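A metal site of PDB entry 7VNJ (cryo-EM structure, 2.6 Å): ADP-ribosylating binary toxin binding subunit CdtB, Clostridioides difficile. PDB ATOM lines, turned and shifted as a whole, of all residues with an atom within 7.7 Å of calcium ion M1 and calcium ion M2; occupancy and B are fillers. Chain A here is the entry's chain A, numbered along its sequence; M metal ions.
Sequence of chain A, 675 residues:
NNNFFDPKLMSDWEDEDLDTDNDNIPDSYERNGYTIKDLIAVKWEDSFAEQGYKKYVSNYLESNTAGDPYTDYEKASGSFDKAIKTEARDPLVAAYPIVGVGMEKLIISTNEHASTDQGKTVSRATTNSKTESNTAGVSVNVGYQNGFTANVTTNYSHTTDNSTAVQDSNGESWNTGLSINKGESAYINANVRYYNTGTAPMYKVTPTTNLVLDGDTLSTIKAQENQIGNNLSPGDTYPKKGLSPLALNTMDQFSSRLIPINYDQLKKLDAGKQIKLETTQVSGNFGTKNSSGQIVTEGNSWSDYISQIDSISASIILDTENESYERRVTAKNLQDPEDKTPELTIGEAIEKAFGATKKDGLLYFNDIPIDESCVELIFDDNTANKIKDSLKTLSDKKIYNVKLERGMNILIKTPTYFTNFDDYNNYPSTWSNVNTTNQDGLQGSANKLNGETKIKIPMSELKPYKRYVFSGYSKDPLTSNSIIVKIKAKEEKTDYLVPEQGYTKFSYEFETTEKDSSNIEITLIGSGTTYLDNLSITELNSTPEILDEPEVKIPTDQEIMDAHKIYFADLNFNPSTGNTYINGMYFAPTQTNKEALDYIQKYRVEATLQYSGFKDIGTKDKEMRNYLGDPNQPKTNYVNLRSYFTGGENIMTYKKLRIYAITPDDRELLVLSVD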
ATOM      1  N   LEU A  18     -19.493  -0.455 -15.370  1.00  0.00           N
ATOM      2  CA  LEU A  18     -18.851   0.134 -14.206  1.00  0.00           C
ATOM      3  C   LEU A  18     -18.888  -0.863 -13.049  1.00  0.00           C
ATOM      4  O   LEU A  18     -19.954  -1.363 -12.691  1.00  0.00           O
ATOM      5  CB  LEU A  18     -19.543   1.434 -13.803  1.00  0.00           C
ATOM      6  CG  LEU A  18     -18.929   2.220 -12.642  1.00  0.00           C
ATOM      7  CD1 LEU A  18     -17.517   2.639 -12.984  1.00  0.00           C
ATOM      8  CD2 LEU A  18     -19.790   3.416 -12.313  1.00  0.00           C
ATOM      9  N   ASP A  19     -17.721  -1.127 -12.471  1.00  0.00           N
ATOM     10  CA  ASP A  19     -17.566  -2.116 -11.399  1.00  0.00           C
ATOM     11  C   ASP A  19     -16.825  -1.436 -10.251  1.00  0.00           C
ATOM     12  O   ASP A  19     -15.588  -1.455 -10.201  1.00  0.00           O
ATOM     13  CB  ASP A  19     -16.831  -3.345 -11.898  1.00  0.00           C
ATOM     14  CG  ASP A  19     -17.014  -4.546 -10.998  1.00  0.00           C
ATOM     15  OD1 ASP A  19     -17.696  -4.415  -9.963  1.00  0.00           O
ATOM     16  OD2 ASP A  19     -16.471  -5.623 -11.321  1.00  0.00           O
ATOM     17  N   THR A  20     -17.567  -0.823  -9.332  1.00  0.00           N
ATOM     18  CA  THR A  20     -16.952  -0.046  -8.269  1.00  0.00           C
ATOM     19  C   THR A  20     -16.188  -0.931  -7.291  1.00  0.00           C
ATOM     20  O   THR A  20     -15.066  -0.597  -6.890  1.00  0.00           O
ATOM     21  CB  THR A  20     -18.010   0.778  -7.533  1.00  0.00           C
ATOM     22  OG1 THR A  20     -18.811   1.484  -8.498  1.00  0.00           O
ATOM     23  CG2 THR A  20     -17.357   1.773  -6.609  1.00  0.00           C
ATOM     24  N   ASP A  21     -16.776  -2.056  -6.894  1.00  0.00           N
ATOM     25  CA  ASP A  21     -16.146  -2.934  -5.914  1.00  0.00           C
ATOM     26  C   ASP A  21     -15.232  -3.972  -6.532  1.00  0.00           C
ATOM     27  O   ASP A  21     -14.564  -4.705  -5.792  1.00  0.00           O
ATOM     28  CB  ASP A  21     -17.218  -3.636  -5.062  1.00  0.00           C
ATOM     29  CG  ASP A  21     -18.259  -4.332  -5.900  1.00  0.00           C
ATOM     30  OD1 ASP A  21     -18.134  -4.340  -7.136  1.00  0.00           O
ATOM     31  OD2 ASP A  21     -19.208  -4.886  -5.319  1.00  0.00           O
ATOM     32  N   ASN A  22     -15.191  -4.059  -7.861  1.00  0.00           N
ATOM     33  CA  ASN A  22     -14.275  -4.956  -8.583  1.00  0.00           C
ATOM     34  C   ASN A  22     -14.546  -6.425  -8.252  1.00  0.00           C
ATOM     35  O   ASN A  22     -13.625  -7.199  -7.993  1.00  0.00           O
ATOM     36  CB  ASN A  22     -12.820  -4.594  -8.300  1.00  0.00           C
ATOM     37  CG  ASN A  22     -12.419  -3.276  -8.934  1.00  0.00           C
ATOM     38  OD1 ASN A  22     -12.442  -3.125 -10.151  1.00  0.00           O
ATOM     39  ND2 ASN A  22     -12.034  -2.311  -8.100  1.00  0.00           N
ATOM     40  N   ASP A  23     -15.820  -6.804  -8.277  1.00  0.00           N
ATOM     41  CA  ASP A  23     -16.203  -8.195  -8.054  1.00  0.00           C
ATOM     42  C   ASP A  23     -16.709  -8.860  -9.328  1.00  0.00           C
ATOM     43  O   ASP A  23     -17.442  -9.858  -9.252  1.00  0.00           O
ATOM     44  CB  ASP A  23     -17.254  -8.282  -6.953  1.00  0.00           C
ATOM     45  CG  ASP A  23     -18.527  -7.523  -7.271  1.00  0.00           C
ATOM     46  OD1 ASP A  23     -18.585  -6.857  -8.319  1.00  0.00           O
ATOM     47  OD2 ASP A  23     -19.469  -7.586  -6.454  1.00  0.00           O
ATOM     48  N   ASN A  24     -16.363  -8.312 -10.497  1.00  0.00           N
ATOM     49  CA  ASN A  24     -16.698  -8.853 -11.814  1.00  0.00           C
ATOM     50  C   ASN A  24     -18.180  -8.739 -12.159  1.00  0.00           C
ATOM     51  O   ASN A  24     -18.618  -9.369 -13.125  1.00  0.00           O
ATOM     52  CB  ASN A  24     -16.250 -10.304 -11.983  1.00  0.00           C
ATOM     53  CG  ASN A  24     -14.751 -10.450 -12.037  1.00  0.00           C
ATOM     54  OD1 ASN A  24     -14.036  -9.528 -12.422  1.00  0.00           O
ATOM     55  ND2 ASN A  24     -14.258 -11.615 -11.638  1.00  0.00           N
ATOM     56  N   ILE A  25     -18.955  -7.979 -11.398  1.00  0.00           N
ATOM     57  CA  ILE A  25     -20.365  -7.755 -11.679  1.00  0.00           C
ATOM     58  C   ILE A  25     -20.592  -6.255 -11.780  1.00  0.00           C
ATOM     59  O   ILE A  25     -20.237  -5.524 -10.849  1.00  0.00           O
ATOM     60  CB  ILE A  25     -21.291  -8.361 -10.609  1.00  0.00           C
ATOM     61  CG1 ILE A  25     -20.855  -9.787 -10.268  1.00  0.00           C
ATOM     62  CG2 ILE A  25     -22.729  -8.365 -11.090  1.00  0.00           C
ATOM     63  CD1 ILE A  25     -21.513 -10.339  -9.036  1.00  0.00           C
ATOM     64  N   PRO A  26     -21.151  -5.748 -12.879  1.00  0.00           N
ATOM     65  CA  PRO A  26     -21.349  -4.303 -12.998  1.00  0.00           C
ATOM     66  C   PRO A  26     -22.340  -3.777 -11.971  1.00  0.00           C
ATOM     67  O   PRO A  26     -23.176  -4.511 -11.446  1.00  0.00           O
ATOM     68  CB  PRO A  26     -21.893  -4.146 -14.425  1.00  0.00           C
ATOM     69  CG  PRO A  26     -21.460  -5.371 -15.145  1.00  0.00           C
ATOM     70  CD  PRO A  26     -21.474  -6.463 -14.122  1.00  0.00           C
ATOM     71  N   ASP A  27     -22.211  -2.479 -11.676  1.00  0.00           N
ATOM     72  CA  ASP A  27     -23.039  -1.866 -10.643  1.00  0.00           C
ATOM     73  C   ASP A  27     -24.521  -1.937 -10.978  1.00  0.00           C
ATOM     74  O   ASP A  27     -25.351  -2.263 -10.127  1.00  0.00           O
ATOM     75  CB  ASP A  27     -22.618  -0.410 -10.437  1.00  0.00           C
ATOM     76  CG  ASP A  27     -21.223  -0.286  -9.854  1.00  0.00           C
ATOM     77  OD1 ASP A  27     -20.608  -1.334  -9.559  1.00  0.00           O
ATOM     78  OD2 ASP A  27     -20.746   0.852  -9.691  1.00  0.00           O
ATOM     79  N   SER A  28     -24.882  -1.636 -12.229  1.00  0.00           N
ATOM     80  CA  SER A  28     -26.278  -1.661 -12.617  1.00  0.00           C
ATOM     81  C   SER A  28     -26.836  -3.079 -12.561  1.00  0.00           C
ATOM     82  O   SER A  28     -28.014  -3.278 -12.217  1.00  0.00           O
ATOM     83  CB  SER A  28     -26.460  -1.074 -14.012  1.00  0.00           C
ATOM     84  OG  SER A  28     -25.640  -1.747 -14.953  1.00  0.00           O
ATOM     85  N   TYR A  29     -26.017  -4.073 -12.901  1.00  0.00           N
ATOM     86  CA  TYR A  29     -26.455  -5.459 -12.802  1.00  0.00           C
ATOM     87  C   TYR A  29     -26.775  -5.824 -11.355  1.00  0.00           C
ATOM     88  O   TYR A  29     -27.791  -6.477 -11.085  1.00  0.00           O
ATOM     89  CB  TYR A  29     -25.385  -6.399 -13.362  1.00  0.00           C
ATOM     90  CG  TYR A  29     -25.236  -6.393 -14.866  1.00  0.00           C
ATOM     91  CD1 TYR A  29     -25.648  -5.304 -15.630  1.00  0.00           C
ATOM     92  CD2 TYR A  29     -24.668  -7.467 -15.521  1.00  0.00           C
ATOM     93  CE1 TYR A  29     -25.500  -5.295 -16.996  1.00  0.00           C
ATOM     94  CE2 TYR A  29     -24.520  -7.471 -16.893  1.00  0.00           C
ATOM     95  CZ  TYR A  29     -24.932  -6.385 -17.624  1.00  0.00           C
ATOM     96  OH  TYR A  29     -24.791  -6.388 -18.984  1.00  0.00           O
ATOM     97  N   GLU A  30     -25.912  -5.420 -10.422  1.00  0.00           N
ATOM     98  CA  GLU A  30     -26.175  -5.697  -9.016  1.00  0.00           C
ATOM     99  C   GLU A  30     -27.415  -4.964  -8.519  1.00  0.00           C
ATOM    100  O   GLU A  30     -28.195  -5.506  -7.733  1.00  0.00           O
ATOM    101  CB  GLU A  30     -24.959  -5.309  -8.167  1.00  0.00           C
ATOM    102  CG  GLU A  30     -23.692  -6.044  -8.516  1.00  0.00           C
ATOM    103  CD  GLU A  30     -22.693  -6.073  -7.367  1.00  0.00           C
ATOM    104  OE1 GLU A  30     -23.031  -6.632  -6.308  1.00  0.00           O
ATOM    105  OE2 GLU A  30     -21.593  -5.526  -7.536  1.00  0.00           O
ATOM    106  N   TYR A  34     -29.494  -9.886 -11.883  1.00  0.00           N
ATOM    107  CA  TYR A  34     -28.604 -10.570 -12.806  1.00  0.00           C
ATOM    108  C   TYR A  34     -28.634 -12.057 -12.529  1.00  0.00           C
ATOM    109  O   TYR A  34     -29.155 -12.513 -11.506  1.00  0.00           O
ATOM    110  CB  TYR A  34     -27.174 -10.039 -12.704  1.00  0.00           C
ATOM    111  CG  TYR A  34     -26.531 -10.267 -11.351  1.00  0.00           C
ATOM    112  CD1 TYR A  34     -26.764  -9.406 -10.295  1.00  0.00           C
ATOM    113  CD2 TYR A  34     -25.703 -11.353 -11.133  1.00  0.00           C
ATOM    114  CE1 TYR A  34     -26.191  -9.611  -9.069  1.00  0.00           C
ATOM    115  CE2 TYR A  34     -25.115 -11.575  -9.904  1.00  0.00           C
ATOM    116  CZ  TYR A  34     -25.363 -10.698  -8.875  1.00  0.00           C
ATOM    117  OH  TYR A  34     -24.789 -10.903  -7.648  1.00  0.00           O
ATOM    118  N   SER A  58     -27.445  -7.686  -5.192  1.00  0.00           N
ATOM    119  CA  SER A  58     -26.387  -7.613  -4.192  1.00  0.00           C
ATOM    120  C   SER A  58     -25.922  -6.170  -4.051  1.00  0.00           C
ATOM    121  O   SER A  58     -26.429  -5.254  -4.696  1.00  0.00           O
ATOM    122  CB  SER A  58     -25.227  -8.542  -4.560  1.00  0.00           C
ATOM    123  OG  SER A  58     -24.612  -8.150  -5.768  1.00  0.00           O
ATOM    124  N   ASN A  59     -24.940  -5.969  -3.174  1.00  0.00           N
ATOM    125  CA  ASN A  59     -24.408  -4.650  -2.873  1.00  0.00           C
ATOM    126  C   ASN A  59     -23.328  -4.293  -3.877  1.00  0.00           C
ATOM    127  O   ASN A  59     -22.298  -4.961  -3.959  1.00  0.00           O
ATOM    128  CB  ASN A  59     -23.856  -4.638  -1.441  1.00  0.00           C
ATOM    129  CG  ASN A  59     -23.544  -3.241  -0.948  1.00  0.00           C
ATOM    130  OD1 ASN A  59     -23.476  -2.294  -1.719  1.00  0.00           O
ATOM    131  ND2 ASN A  59     -23.366  -3.117   0.358  1.00  0.00           N
ATOM    132  N   TYR A  60     -23.550  -3.228  -4.641  1.00  0.00           N
ATOM    133  CA  TYR A  60     -22.604  -2.832  -5.670  1.00  0.00           C
ATOM    134  C   TYR A  60     -21.398  -2.078  -5.120  1.00  0.00           C
ATOM    135  O   TYR A  60     -20.435  -1.875  -5.856  1.00  0.00           O
ATOM    136  CB  TYR A  60     -23.297  -1.991  -6.741  1.00  0.00           C
ATOM    137  CG  TYR A  60     -23.600  -0.560  -6.352  1.00  0.00           C
ATOM    138  CD1 TYR A  60     -24.737  -0.252  -5.613  1.00  0.00           C
ATOM    139  CD2 TYR A  60     -22.771   0.477  -6.738  1.00  0.00           C
ATOM    140  CE1 TYR A  60     -25.018   1.047  -5.264  1.00  0.00           C
ATOM    141  CE2 TYR A  60     -23.045   1.782  -6.385  1.00  0.00           C
ATOM    142  CZ  TYR A  60     -24.169   2.061  -5.652  1.00  0.00           C
ATOM    143  OH  TYR A  60     -24.450   3.360  -5.303  1.00  0.00           O
ATOM    144  N   LEU A  61     -21.437  -1.679  -3.854  1.00  0.00           N
ATOM    145  CA  LEU A  61     -20.295  -1.042  -3.198  1.00  0.00           C
ATOM    146  C   LEU A  61     -19.530  -1.993  -2.305  1.00  0.00           C
ATOM    147  O   LEU A  61     -18.545  -1.579  -1.687  1.00  0.00           O
ATOM    148  CB  LEU A  61     -20.765   0.169  -2.383  1.00  0.00           C
ATOM    149  CG  LEU A  61     -21.127   1.419  -3.158  1.00  0.00           C
ATOM    150  CD1 LEU A  61     -21.514   2.538  -2.210  1.00  0.00           C
ATOM    151  CD2 LEU A  61     -19.971   1.858  -4.034  1.00  0.00           C
ATOM    152  N   GLU A  62     -19.939  -3.253  -2.225  1.00  0.00           N
ATOM    153  CA  GLU A  62     -19.316  -4.221  -1.331  1.00  0.00           C
ATOM    154  C   GLU A  62     -19.009  -5.497  -2.105  1.00  0.00           C
ATOM    155  O   GLU A  62     -19.881  -6.029  -2.800  1.00  0.00           O
ATOM    156  CB  GLU A  62     -20.234  -4.527  -0.146  1.00  0.00           C
ATOM    157  CG  GLU A  62     -19.640  -5.483   0.870  1.00  0.00           C
ATOM    158  CD  GLU A  62     -18.499  -4.864   1.642  1.00  0.00           C
ATOM    159  OE1 GLU A  62     -18.597  -3.679   2.020  1.00  0.00           O
ATOM    160  OE2 GLU A  62     -17.493  -5.577   1.879  1.00  0.00           O
ATOM    161  N   SER A  63     -17.775  -5.984  -1.977  1.00  0.00           N
ATOM    162  CA  SER A  63     -17.377  -7.190  -2.686  1.00  0.00           C
ATOM    163  C   SER A  63     -17.968  -8.445  -2.063  1.00  0.00           C
ATOM    164  O   SER A  63     -18.191  -9.432  -2.759  1.00  0.00           O
ATOM    165  CB  SER A  63     -15.856  -7.284  -2.732  1.00  0.00           C
ATOM    166  OG  SER A  63     -15.442  -8.367  -3.544  1.00  0.00           O
ATOM    167  N   ASN A  64     -18.214  -8.423  -0.751  1.00  0.00           N
ATOM    168  CA  ASN A  64     -18.792  -9.552  -0.034  1.00  0.00           C
ATOM    169  C   ASN A  64     -20.041  -9.031   0.675  1.00  0.00           C
ATOM    170  O   ASN A  64     -19.973  -8.542   1.798  1.00  0.00           O
ATOM    171  CB  ASN A  64     -17.793 -10.141   0.955  1.00  0.00           C
ATOM    172  CG  ASN A  64     -16.537 -10.646   0.289  1.00  0.00           C
ATOM    173  OD1 ASN A  64     -15.792  -9.877  -0.311  1.00  0.00           O
ATOM    174  ND2 ASN A  64     -16.274 -11.940   0.415  1.00  0.00           N
ATOM    175  N   THR A  65     -21.188  -9.159   0.000  1.00  0.00           N
ATOM    176  CA  THR A  65     -22.421  -8.591   0.541  1.00  0.00           C
ATOM    177  C   THR A  65     -22.805  -9.240   1.870  1.00  0.00           C
ATOM    178  O   THR A  65     -23.193  -8.544   2.817  1.00  0.00           O
ATOM    179  CB  THR A  65     -23.557  -8.763  -0.471  1.00  0.00           C
ATOM    180  OG1 THR A  65     -23.161  -8.206  -1.726  1.00  0.00           O
ATOM    181  CG2 THR A  65     -24.804  -8.049   0.015  1.00  0.00           C
ATOM    182  N   THR A  71     -16.829 -14.024  -2.308  1.00  0.00           N
ATOM    183  CA  THR A  71     -17.319 -12.818  -2.948  1.00  0.00           C
ATOM    184  C   THR A  71     -18.672 -13.065  -3.602  1.00  0.00           C
ATOM    185  O   THR A  71     -19.149 -14.204  -3.707  1.00  0.00           O
ATOM    186  CB  THR A  71     -16.317 -12.307  -3.980  1.00  0.00           C
ATOM    187  OG1 THR A  71     -16.400 -13.104  -5.164  1.00  0.00           O
ATOM    188  CG2 THR A  71     -14.908 -12.390  -3.434  1.00  0.00           C
ATOM    189  N   ASP A  72     -19.299 -11.974  -4.057  1.00  0.00           N
ATOM    190  CA  ASP A  72     -20.608 -12.081  -4.699  1.00  0.00           C
ATOM    191  C   ASP A  72     -20.536 -12.932  -5.958  1.00  0.00           C
ATOM    192  O   ASP A  72     -21.407 -13.791  -6.184  1.00  0.00           O
ATOM    193  CB  ASP A  72     -21.144 -10.700  -5.020  1.00  0.00           C
ATOM    194  CG  ASP A  72     -21.464  -9.896  -3.779  1.00  0.00           C
ATOM    195  OD1 ASP A  72     -21.478 -10.475  -2.683  1.00  0.00           O
ATOM    196  OD2 ASP A  72     -21.691  -8.677  -3.902  1.00  0.00           O
ATOM    197  N   TYR A  73     -19.522 -12.715  -6.789  1.00  0.00           N
ATOM    198  CA  TYR A  73     -19.400 -13.494  -8.018  1.00  0.00           C
ATOM    199  C   TYR A  73     -19.148 -14.963  -7.715  1.00  0.00           C
ATOM    200  O   TYR A  73     -19.732 -15.840  -8.363  1.00  0.00           O
ATOM    201  CB  TYR A  73     -18.279 -12.934  -8.893  1.00  0.00           C
ATOM    202  CG  TYR A  73     -17.995 -13.804 -10.091  1.00  0.00           C
ATOM    203  CD1 TYR A  73     -18.825 -13.778 -11.205  1.00  0.00           C
ATOM    204  CD2 TYR A  73     -16.909 -14.674 -10.104  1.00  0.00           C
ATOM    205  CE1 TYR A  73     -18.570 -14.579 -12.295  1.00  0.00           C
ATOM    206  CE2 TYR A  73     -16.661 -15.487 -11.189  1.00  0.00           C
ATOM    207  CZ  TYR A  73     -17.492 -15.424 -12.282  1.00  0.00           C
ATOM    208  OH  TYR A  73     -17.244 -16.219 -13.368  1.00  0.00           O
ATOM    209  N   PRO A  91     -26.092 -13.954  -3.039  1.00  0.00           N
ATOM    210  CA  PRO A  91     -25.241 -13.090  -2.198  1.00  0.00           C
ATOM    211  C   PRO A  91     -25.854 -12.687  -0.869  1.00  0.00           C
ATOM    212  O   PRO A  91     -25.111 -12.264   0.017  1.00  0.00           O
ATOM    213  CB  PRO A  91     -25.008 -11.866  -3.096  1.00  0.00           C
ATOM    214  CG  PRO A  91     -25.131 -12.403  -4.478  1.00  0.00           C
ATOM    215  CD  PRO A  91     -26.210 -13.435  -4.414  1.00  0.00           C
HETATM  216 CA    CA M   1     -20.881  -6.609  -4.863  1.00  0.00          CA
HETATM  217 CA    CA M   2     -19.746  -4.706  -8.749  1.00  0.00          CA
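Calcium ion M2 is bound by the backbone carbonyl oxygen of Ile 25 (2.3 Å), the side-chain carboxylate of Asp 21 (2.3 Å), the side-chain carboxylate of Glu 30 (2.4 Å), the side-chain carboxylate of Asp 19 (2.4 Å) and the side-chain carboxylate of Asp 23 (2.5 Å).
Within 4 Å of calcium ion M1: Asp 21, Asp 23, Glu 30, Asn 59, Glu 62 and Asp 72.
The nearest printed residue that does not touch calcium ion M1 is Ser 58 (4.1 Å).
Residues that only touch calcium ion M2: Asp 27.
Six residues have an atom within 4 Å of calcium ion M2: Asp 19, Asp 21, Asp 23, Ile 25, Asp 27 and Glu 30.
The nearest printed residue that does not touch calcium ion M2 is Tyr 60 (4.1 Å).
O of Ser 63 lies within hydrogen-bond range of N of Asp 72, 3.1 Å away.
The backbone NH (N) of Asn 24 lies within hydrogen-bond range of the side-chain carboxylate (OD2) of Asp 19.
The backbone NH (N) of Asp 27 is in hydrogen-bond range of the backbone carbonyl oxygen (O) of Leu 18 (2.7 Å).
The backbone NH (N) of Asn 22 sits close to the side-chain carboxylate (OD1) of Asp 19, 3.3 Å away.
OD1 of Asp 27 sits at hydrogen-bond distance from N of Thr 20 (3.1 Å).
N of Leu 61 sits at hydrogen-bond distance from OD1 of Asn 59, 3.0 Å away.
The backbone NH of Asn 59 lies within hydrogen-bond range of the side-chain hydroxyl of Thr 65 (3.2 Å).
The backbone carbonyl oxygen (O) of Glu 30 sits at hydrogen-bond distance from the backbone NH (N) of Ser 58, at 3.4 Å.
OD2 of Asp 23 is bound to calcium ion M1 (2.3 Å).
Calcium ion M1 is bound by the backbone carbonyl oxygen (O) of Asn 59, at 2.4 Å.
Calcium ion M1 is bound by the backbone carbonyl oxygen (O) of Glu 62 (2.4 Å).
Calcium ion M1 is bound by the side-chain carboxylate (OD2) of Asp 72 (2.4 Å).
Calcium ion M1 is bound by OD2 of Asp 21 (2.4 Å).
OE1 of Glu 30 binds calcium ion M1.
Slightly farther from calcium ion M1 lies OE2 of Glu 30 (3.0 Å).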
